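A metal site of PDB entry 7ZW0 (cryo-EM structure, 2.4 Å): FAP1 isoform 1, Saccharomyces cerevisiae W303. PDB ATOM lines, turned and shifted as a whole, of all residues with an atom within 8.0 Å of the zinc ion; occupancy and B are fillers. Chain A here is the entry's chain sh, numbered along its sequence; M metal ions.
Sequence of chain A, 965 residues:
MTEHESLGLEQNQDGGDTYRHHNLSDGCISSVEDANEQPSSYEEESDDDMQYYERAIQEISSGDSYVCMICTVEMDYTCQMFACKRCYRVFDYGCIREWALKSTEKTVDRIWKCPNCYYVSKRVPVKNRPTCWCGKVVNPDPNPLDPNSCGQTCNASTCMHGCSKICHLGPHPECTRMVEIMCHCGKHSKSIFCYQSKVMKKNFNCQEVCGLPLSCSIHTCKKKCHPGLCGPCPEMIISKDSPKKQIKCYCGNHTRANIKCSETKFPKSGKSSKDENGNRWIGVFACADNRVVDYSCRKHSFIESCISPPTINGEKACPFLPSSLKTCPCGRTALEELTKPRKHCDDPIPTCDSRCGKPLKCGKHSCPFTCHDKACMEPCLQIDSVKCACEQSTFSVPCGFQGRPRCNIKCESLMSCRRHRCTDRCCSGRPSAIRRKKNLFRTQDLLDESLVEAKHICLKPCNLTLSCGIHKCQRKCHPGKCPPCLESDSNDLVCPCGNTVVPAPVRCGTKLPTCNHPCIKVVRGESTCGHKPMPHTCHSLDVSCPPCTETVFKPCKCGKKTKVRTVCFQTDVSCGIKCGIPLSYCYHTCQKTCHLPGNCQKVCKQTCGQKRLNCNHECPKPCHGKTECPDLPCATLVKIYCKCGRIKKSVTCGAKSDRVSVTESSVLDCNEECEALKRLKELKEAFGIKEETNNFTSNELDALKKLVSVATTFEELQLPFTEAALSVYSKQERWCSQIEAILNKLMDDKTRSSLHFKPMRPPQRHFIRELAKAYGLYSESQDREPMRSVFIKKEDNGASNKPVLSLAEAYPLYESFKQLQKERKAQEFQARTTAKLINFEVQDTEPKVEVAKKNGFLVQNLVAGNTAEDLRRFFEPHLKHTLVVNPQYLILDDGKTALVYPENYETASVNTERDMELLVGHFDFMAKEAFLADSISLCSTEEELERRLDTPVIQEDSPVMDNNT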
ATOM      1  N   MET A  69      29.900 -30.764 -30.777  1.00  0.00           N
ATOM      2  CA  MET A  69      30.479 -29.938 -29.717  1.00  0.00           C
ATOM      3  C   MET A  69      30.672 -30.589 -28.355  1.00  0.00           C
ATOM      4  O   MET A  69      31.712 -30.401 -27.728  1.00  0.00           O
ATOM      5  CB  MET A  69      29.675 -28.646 -29.568  1.00  0.00           C
ATOM      6  CG  MET A  69      29.716 -27.766 -30.802  1.00  0.00           C
ATOM      7  SD  MET A  69      28.920 -26.160 -30.580  1.00  0.00           S
ATOM      8  CE  MET A  69      29.954 -25.445 -29.306  1.00  0.00           C
ATOM      9  N   PHE A  82      21.782 -32.956 -34.313  1.00  0.00           N
ATOM     10  CA  PHE A  82      20.728 -32.123 -33.714  1.00  0.00           C
ATOM     11  C   PHE A  82      20.901 -30.657 -34.122  1.00  0.00           C
ATOM     12  O   PHE A  82      22.020 -30.142 -34.087  1.00  0.00           O
ATOM     13  CB  PHE A  82      20.753 -32.225 -32.205  1.00  0.00           C
ATOM     14  CG  PHE A  82      19.744 -31.338 -31.526  1.00  0.00           C
ATOM     15  CD1 PHE A  82      18.411 -31.694 -31.500  1.00  0.00           C
ATOM     16  CD2 PHE A  82      20.134 -30.168 -30.910  1.00  0.00           C
ATOM     17  CE1 PHE A  82      17.471 -30.885 -30.880  1.00  0.00           C
ATOM     18  CE2 PHE A  82      19.211 -29.347 -30.299  1.00  0.00           C
ATOM     19  CZ  PHE A  82      17.882 -29.712 -30.275  1.00  0.00           C
ATOM     20  N   ALA A  83      19.824 -29.999 -34.517  1.00  0.00           N
ATOM     21  CA  ALA A  83      19.922 -28.620 -34.980  1.00  0.00           C
ATOM     22  C   ALA A  83      19.155 -27.656 -34.102  1.00  0.00           C
ATOM     23  O   ALA A  83      18.029 -27.937 -33.692  1.00  0.00           O
ATOM     24  CB  ALA A  83      19.470 -28.513 -36.420  1.00  0.00           C
ATOM     25  N   CYS A  84      19.749 -26.509 -33.816  1.00  0.00           N
ATOM     26  CA  CYS A  84      19.062 -25.492 -33.032  1.00  0.00           C
ATOM     27  C   CYS A  84      18.896 -24.272 -33.904  1.00  0.00           C
ATOM     28  O   CYS A  84      19.848 -23.850 -34.543  1.00  0.00           O
ATOM     29  CB  CYS A  84      19.844 -25.134 -31.769  1.00  0.00           C
ATOM     30  SG  CYS A  84      19.187 -23.720 -30.866  1.00  0.00           S
ATOM     31  N   LYS A  85      17.705 -23.698 -33.943  1.00  0.00           N
ATOM     32  CA  LYS A  85      17.466 -22.573 -34.831  1.00  0.00           C
ATOM     33  C   LYS A  85      18.325 -21.377 -34.474  1.00  0.00           C
ATOM     34  O   LYS A  85      18.833 -20.692 -35.349  1.00  0.00           O
ATOM     35  CB  LYS A  85      15.979 -22.175 -34.811  1.00  0.00           C
ATOM     36  CG  LYS A  85      15.061 -23.077 -35.637  1.00  0.00           C
ATOM     37  CD  LYS A  85      14.674 -24.352 -34.896  1.00  0.00           C
ATOM     38  CE  LYS A  85      15.353 -25.568 -35.484  1.00  0.00           C
ATOM     39  NZ  LYS A  85      15.244 -26.748 -34.582  1.00  0.00           N
ATOM     40  N   ARG A  86      18.503 -21.124 -33.186  1.00  0.00           N
ATOM     41  CA  ARG A  86      19.257 -19.953 -32.769  1.00  0.00           C
ATOM     42  C   ARG A  86      20.721 -19.999 -33.228  1.00  0.00           C
ATOM     43  O   ARG A  86      21.249 -18.995 -33.713  1.00  0.00           O
ATOM     44  CB  ARG A  86      19.164 -19.774 -31.249  1.00  0.00           C
ATOM     45  CG  ARG A  86      19.545 -18.379 -30.772  1.00  0.00           C
ATOM     46  CD  ARG A  86      18.600 -17.333 -31.329  1.00  0.00           C
ATOM     47  NE  ARG A  86      19.157 -15.986 -31.247  1.00  0.00           N
ATOM     48  CZ  ARG A  86      19.849 -15.399 -32.220  1.00  0.00           C
ATOM     49  NH1 ARG A  86      20.062 -16.040 -33.357  1.00  0.00           N
ATOM     50  NH2 ARG A  86      20.328 -14.172 -32.056  1.00  0.00           N
ATOM     51  N   CYS A  87      21.364 -21.151 -33.098  1.00  0.00           N
ATOM     52  CA  CYS A  87      22.760 -21.266 -33.516  1.00  0.00           C
ATOM     53  C   CYS A  87      22.961 -21.899 -34.876  1.00  0.00           C
ATOM     54  O   CYS A  87      24.069 -21.844 -35.412  1.00  0.00           O
ATOM     55  CB  CYS A  87      23.542 -22.086 -32.498  1.00  0.00           C
ATOM     56  SG  CYS A  87      23.120 -23.841 -32.505  1.00  0.00           S
ATOM     57  N   TYR A  88      21.914 -22.462 -35.455  1.00  0.00           N
ATOM     58  CA  TYR A  88      22.045 -23.190 -36.719  1.00  0.00           C
ATOM     59  C   TYR A  88      23.335 -23.996 -36.802  1.00  0.00           C
ATOM     60  O   TYR A  88      24.046 -23.949 -37.812  1.00  0.00           O
ATOM     61  CB  TYR A  88      21.857 -22.268 -37.925  1.00  0.00           C
ATOM     62  CG  TYR A  88      20.400 -22.035 -38.235  1.00  0.00           C
ATOM     63  CD1 TYR A  88      19.532 -23.113 -38.363  1.00  0.00           C
ATOM     64  CD2 TYR A  88      19.899 -20.761 -38.408  1.00  0.00           C
ATOM     65  CE1 TYR A  88      18.193 -22.914 -38.645  1.00  0.00           C
ATOM     66  CE2 TYR A  88      18.565 -20.549 -38.687  1.00  0.00           C
ATOM     67  CZ  TYR A  88      17.710 -21.634 -38.797  1.00  0.00           C
ATOM     68  OH  TYR A  88      16.381 -21.431 -39.078  1.00  0.00           O
ATOM     69  N   ARG A  89      23.637 -24.751 -35.751  1.00  0.00           N
ATOM     70  CA  ARG A  89      24.833 -25.565 -35.719  1.00  0.00           C
ATOM     71  C   ARG A  89      24.415 -26.989 -35.374  1.00  0.00           C
ATOM     72  O   ARG A  89      23.360 -27.193 -34.768  1.00  0.00           O
ATOM     73  CB  ARG A  89      25.810 -24.990 -34.685  1.00  0.00           C
ATOM     74  CG  ARG A  89      26.859 -25.934 -34.122  1.00  0.00           C
ATOM     75  CD  ARG A  89      28.226 -25.696 -34.734  1.00  0.00           C
ATOM     76  NE  ARG A  89      29.197 -26.692 -34.291  1.00  0.00           N
ATOM     77  CZ  ARG A  89      30.493 -26.675 -34.607  1.00  0.00           C
ATOM     78  NH1 ARG A  89      30.972 -25.697 -35.360  1.00  0.00           N
ATOM     79  NH2 ARG A  89      31.296 -27.633 -34.169  1.00  0.00           N
ATOM     80  N   VAL A  90      25.209 -27.980 -35.748  1.00  0.00           N
ATOM     81  CA  VAL A  90      24.849 -29.374 -35.502  1.00  0.00           C
ATOM     82  C   VAL A  90      25.791 -30.141 -34.582  1.00  0.00           C
ATOM     83  O   VAL A  90      27.019 -30.003 -34.678  1.00  0.00           O
ATOM     84  CB  VAL A  90      24.629 -30.118 -36.825  1.00  0.00           C
ATOM     85  CG1 VAL A  90      24.935 -31.591 -36.714  1.00  0.00           C
ATOM     86  CG2 VAL A  90      23.212 -29.896 -37.303  1.00  0.00           C
ATOM     87  N   PHE A  91      25.235 -30.912 -33.651  1.00  0.00           N
ATOM     88  CA  PHE A  91      26.048 -31.713 -32.744  1.00  0.00           C
ATOM     89  C   PHE A  91      25.502 -33.121 -32.839  1.00  0.00           C
ATOM     90  O   PHE A  91      24.446 -33.329 -33.418  1.00  0.00           O
ATOM     91  CB  PHE A  91      25.900 -31.208 -31.309  1.00  0.00           C
ATOM     92  CG  PHE A  91      25.297 -29.842 -31.205  1.00  0.00           C
ATOM     93  CD1 PHE A  91      23.914 -29.684 -31.156  1.00  0.00           C
ATOM     94  CD2 PHE A  91      26.098 -28.714 -31.156  1.00  0.00           C
ATOM     95  CE1 PHE A  91      23.354 -28.419 -31.063  1.00  0.00           C
ATOM     96  CE2 PHE A  91      25.544 -27.459 -31.055  1.00  0.00           C
ATOM     97  CZ  PHE A  91      24.165 -27.308 -31.018  1.00  0.00           C
ATOM     98  N   ILE A  96      24.359 -34.228 -27.470  1.00  0.00           N
ATOM     99  CA  ILE A  96      23.684 -33.023 -27.027  1.00  0.00           C
ATOM    100  C   ILE A  96      22.576 -33.347 -26.015  1.00  0.00           C
ATOM    101  O   ILE A  96      22.284 -32.527 -25.144  1.00  0.00           O
ATOM    102  CB  ILE A  96      23.146 -32.193 -28.216  1.00  0.00           C
ATOM    103  CG1 ILE A  96      22.949 -30.728 -27.813  1.00  0.00           C
ATOM    104  CG2 ILE A  96      21.832 -32.750 -28.752  1.00  0.00           C
ATOM    105  CD1 ILE A  96      24.223 -30.042 -27.382  1.00  0.00           C
ATOM    106  N   TRP A 112      17.208 -26.957 -20.621  1.00  0.00           N
ATOM    107  CA  TRP A 112      18.402 -27.355 -21.364  1.00  0.00           C
ATOM    108  C   TRP A 112      19.044 -26.173 -22.104  1.00  0.00           C
ATOM    109  O   TRP A 112      18.346 -25.265 -22.525  1.00  0.00           O
ATOM    110  CB  TRP A 112      18.062 -28.490 -22.332  1.00  0.00           C
ATOM    111  CG  TRP A 112      17.898 -28.076 -23.753  1.00  0.00           C
ATOM    112  CD1 TRP A 112      16.784 -27.559 -24.337  1.00  0.00           C
ATOM    113  CD2 TRP A 112      18.896 -28.156 -24.791  1.00  0.00           C
ATOM    114  NE1 TRP A 112      17.025 -27.316 -25.666  1.00  0.00           N
ATOM    115  CE2 TRP A 112      18.313 -27.668 -25.965  1.00  0.00           C
ATOM    116  CE3 TRP A 112      20.223 -28.593 -24.822  1.00  0.00           C
ATOM    117  CZ2 TRP A 112      19.003 -27.602 -27.164  1.00  0.00           C
ATOM    118  CZ3 TRP A 112      20.900 -28.525 -26.010  1.00  0.00           C
ATOM    119  CH2 TRP A 112      20.304 -28.035 -27.173  1.00  0.00           C
ATOM    120  N   LYS A 113      20.369 -26.185 -22.274  1.00  0.00           N
ATOM    121  CA  LYS A 113      21.042 -25.033 -22.909  1.00  0.00           C
ATOM    122  C   LYS A 113      21.806 -25.413 -24.170  1.00  0.00           C
ATOM    123  O   LYS A 113      22.470 -26.437 -24.199  1.00  0.00           O
ATOM    124  CB  LYS A 113      21.997 -24.370 -21.908  1.00  0.00           C
ATOM    125  CG  LYS A 113      22.549 -23.031 -22.378  1.00  0.00           C
ATOM    126  CD  LYS A 113      23.074 -22.224 -21.207  1.00  0.00           C
ATOM    127  CE  LYS A 113      23.265 -20.773 -21.609  1.00  0.00           C
ATOM    128  NZ  LYS A 113      23.619 -19.922 -20.433  1.00  0.00           N
ATOM    129  N   CYS A 114      21.717 -24.593 -25.197  1.00  0.00           N
ATOM    130  CA  CYS A 114      22.459 -24.855 -26.413  1.00  0.00           C
ATOM    131  C   CYS A 114      23.761 -24.086 -26.386  1.00  0.00           C
ATOM    132  O   CYS A 114      23.749 -22.862 -26.324  1.00  0.00           O
ATOM    133  CB  CYS A 114      21.645 -24.460 -27.637  1.00  0.00           C
ATOM    134  SG  CYS A 114      22.483 -24.815 -29.193  1.00  0.00           S
ATOM    135  N   PRO A 115      24.900 -24.782 -26.450  1.00  0.00           N
ATOM    136  CA  PRO A 115      26.210 -24.124 -26.323  1.00  0.00           C
ATOM    137  C   PRO A 115      26.623 -23.131 -27.407  1.00  0.00           C
ATOM    138  O   PRO A 115      27.179 -22.089 -27.059  1.00  0.00           O
ATOM    139  CB  PRO A 115      27.202 -25.295 -26.344  1.00  0.00           C
ATOM    140  CG  PRO A 115      26.385 -26.519 -26.054  1.00  0.00           C
ATOM    141  CD  PRO A 115      25.034 -26.240 -26.625  1.00  0.00           C
ATOM    142  N   ASN A 116      26.376 -23.427 -28.671  1.00  0.00           N
ATOM    143  CA  ASN A 116      26.866 -22.538 -29.728  1.00  0.00           C
ATOM    144  C   ASN A 116      26.257 -21.155 -29.660  1.00  0.00           C
ATOM    145  O   ASN A 116      26.957 -20.151 -29.826  1.00  0.00           O
ATOM    146  CB  ASN A 116      26.640 -23.157 -31.108  1.00  0.00           C
ATOM    147  CG  ASN A 116      27.533 -22.532 -32.174  1.00  0.00           C
ATOM    148  OD1 ASN A 116      28.755 -22.477 -32.010  1.00  0.00           O
ATOM    149  ND2 ASN A 116      26.933 -22.084 -33.263  1.00  0.00           N
ATOM    150  N   CYS A 117      24.959 -21.077 -29.406  1.00  0.00           N
ATOM    151  CA  CYS A 117      24.312 -19.781 -29.253  1.00  0.00           C
ATOM    152  C   CYS A 117      24.272 -19.396 -27.796  1.00  0.00           C
ATOM    153  O   CYS A 117      23.746 -18.330 -27.458  1.00  0.00           O
ATOM    154  CB  CYS A 117      22.901 -19.815 -29.823  1.00  0.00           C
ATOM    155  SG  CYS A 117      21.986 -21.299 -29.387  1.00  0.00           S
ATOM    156  N   TYR A 118      24.799 -20.253 -26.928  1.00  0.00           N
ATOM    157  CA  TYR A 118      24.755 -20.005 -25.489  1.00  0.00           C
ATOM    158  C   TYR A 118      23.333 -19.620 -25.147  1.00  0.00           C
ATOM    159  O   TYR A 118      23.098 -18.655 -24.424  1.00  0.00           O
ATOM    160  CB  TYR A 118      25.753 -18.906 -25.086  1.00  0.00           C
ATOM    161  CG  TYR A 118      26.181 -18.968 -23.647  1.00  0.00           C
ATOM    162  CD1 TYR A 118      26.819 -20.093 -23.133  1.00  0.00           C
ATOM    163  CD2 TYR A 118      25.960 -17.897 -22.790  1.00  0.00           C
ATOM    164  CE1 TYR A 118      27.207 -20.150 -21.814  1.00  0.00           C
ATOM    165  CE2 TYR A 118      26.352 -17.941 -21.468  1.00  0.00           C
ATOM    166  CZ  TYR A 118      26.985 -19.073 -20.986  1.00  0.00           C
ATOM    167  OH  TYR A 118      27.382 -19.126 -19.666  1.00  0.00           O
ATOM    168  N   TYR A 119      22.371 -20.369 -25.675  1.00  0.00           N
ATOM    169  CA  TYR A 119      20.968 -20.025 -25.466  1.00  0.00           C
ATOM    170  C   TYR A 119      20.222 -21.151 -24.813  1.00  0.00           C
ATOM    171  O   TYR A 119      20.271 -22.289 -25.277  1.00  0.00           O
ATOM    172  CB  TYR A 119      20.342 -19.606 -26.805  1.00  0.00           C
ATOM    173  CG  TYR A 119      18.954 -20.137 -27.118  1.00  0.00           C
ATOM    174  CD1 TYR A 119      18.779 -21.342 -27.781  1.00  0.00           C
ATOM    175  CD2 TYR A 119      17.822 -19.400 -26.801  1.00  0.00           C
ATOM    176  CE1 TYR A 119      17.524 -21.826 -28.080  1.00  0.00           C
ATOM    177  CE2 TYR A 119      16.562 -19.876 -27.098  1.00  0.00           C
ATOM    178  CZ  TYR A 119      16.420 -21.081 -27.731  1.00  0.00           C
ATOM    179  OH  TYR A 119      15.165 -21.566 -28.031  1.00  0.00           O
ATOM    180  N   VAL A 120      19.551 -20.861 -23.706  1.00  0.00           N
ATOM    181  CA  VAL A 120      18.762 -21.886 -23.041  1.00  0.00           C
ATOM    182  C   VAL A 120      17.446 -22.102 -23.753  1.00  0.00           C
ATOM    183  O   VAL A 120      16.852 -21.164 -24.265  1.00  0.00           O
ATOM    184  CB  VAL A 120      18.479 -21.494 -21.583  1.00  0.00           C
ATOM    185  CG1 VAL A 120      19.031 -22.554 -20.634  1.00  0.00           C
ATOM    186  CG2 VAL A 120      19.089 -20.145 -21.277  1.00  0.00           C
ATOM    187  N   SER A 121      16.972 -23.335 -23.776  1.00  0.00           N
ATOM    188  CA  SER A 121      15.673 -23.638 -24.374  1.00  0.00           C
ATOM    189  C   SER A 121      14.911 -24.478 -23.377  1.00  0.00           C
ATOM    190  O   SER A 121      15.509 -24.989 -22.422  1.00  0.00           O
ATOM    191  CB  SER A 121      15.822 -24.323 -25.732  1.00  0.00           C
ATOM    192  OG  SER A 121      14.559 -24.519 -26.351  1.00  0.00           O
HETATM  193 ZN    ZN M   1      21.693 -23.571 -30.615  1.00  0.00          ZN
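The backbone NH (N) of Cys 114 sits at hydrogen-bond distance from the backbone carbonyl oxygen (O) of Tyr 119, 2.7 Å away.
The side-chain sulfur of Cys 87 sits close to the backbone NH of Arg 89.
The side-chain sulfur of Cys 84 lies close to the backbone NH of Arg 86 (3.5 Å).
Four residues have an atom within 4 Å of the zinc ion: Cys 84, Cys 87, Cys 114 and Cys 117.
Along chain A the residues within 4 Å of the zinc ion span positions 84 to 117.
The zinc ion is bound by SG of Cys 114 (2.0 Å), SG of Cys 87 (2.4 Å), SG of Cys 84 (2.5 Å) and SG of Cys 117 (2.6 Å).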
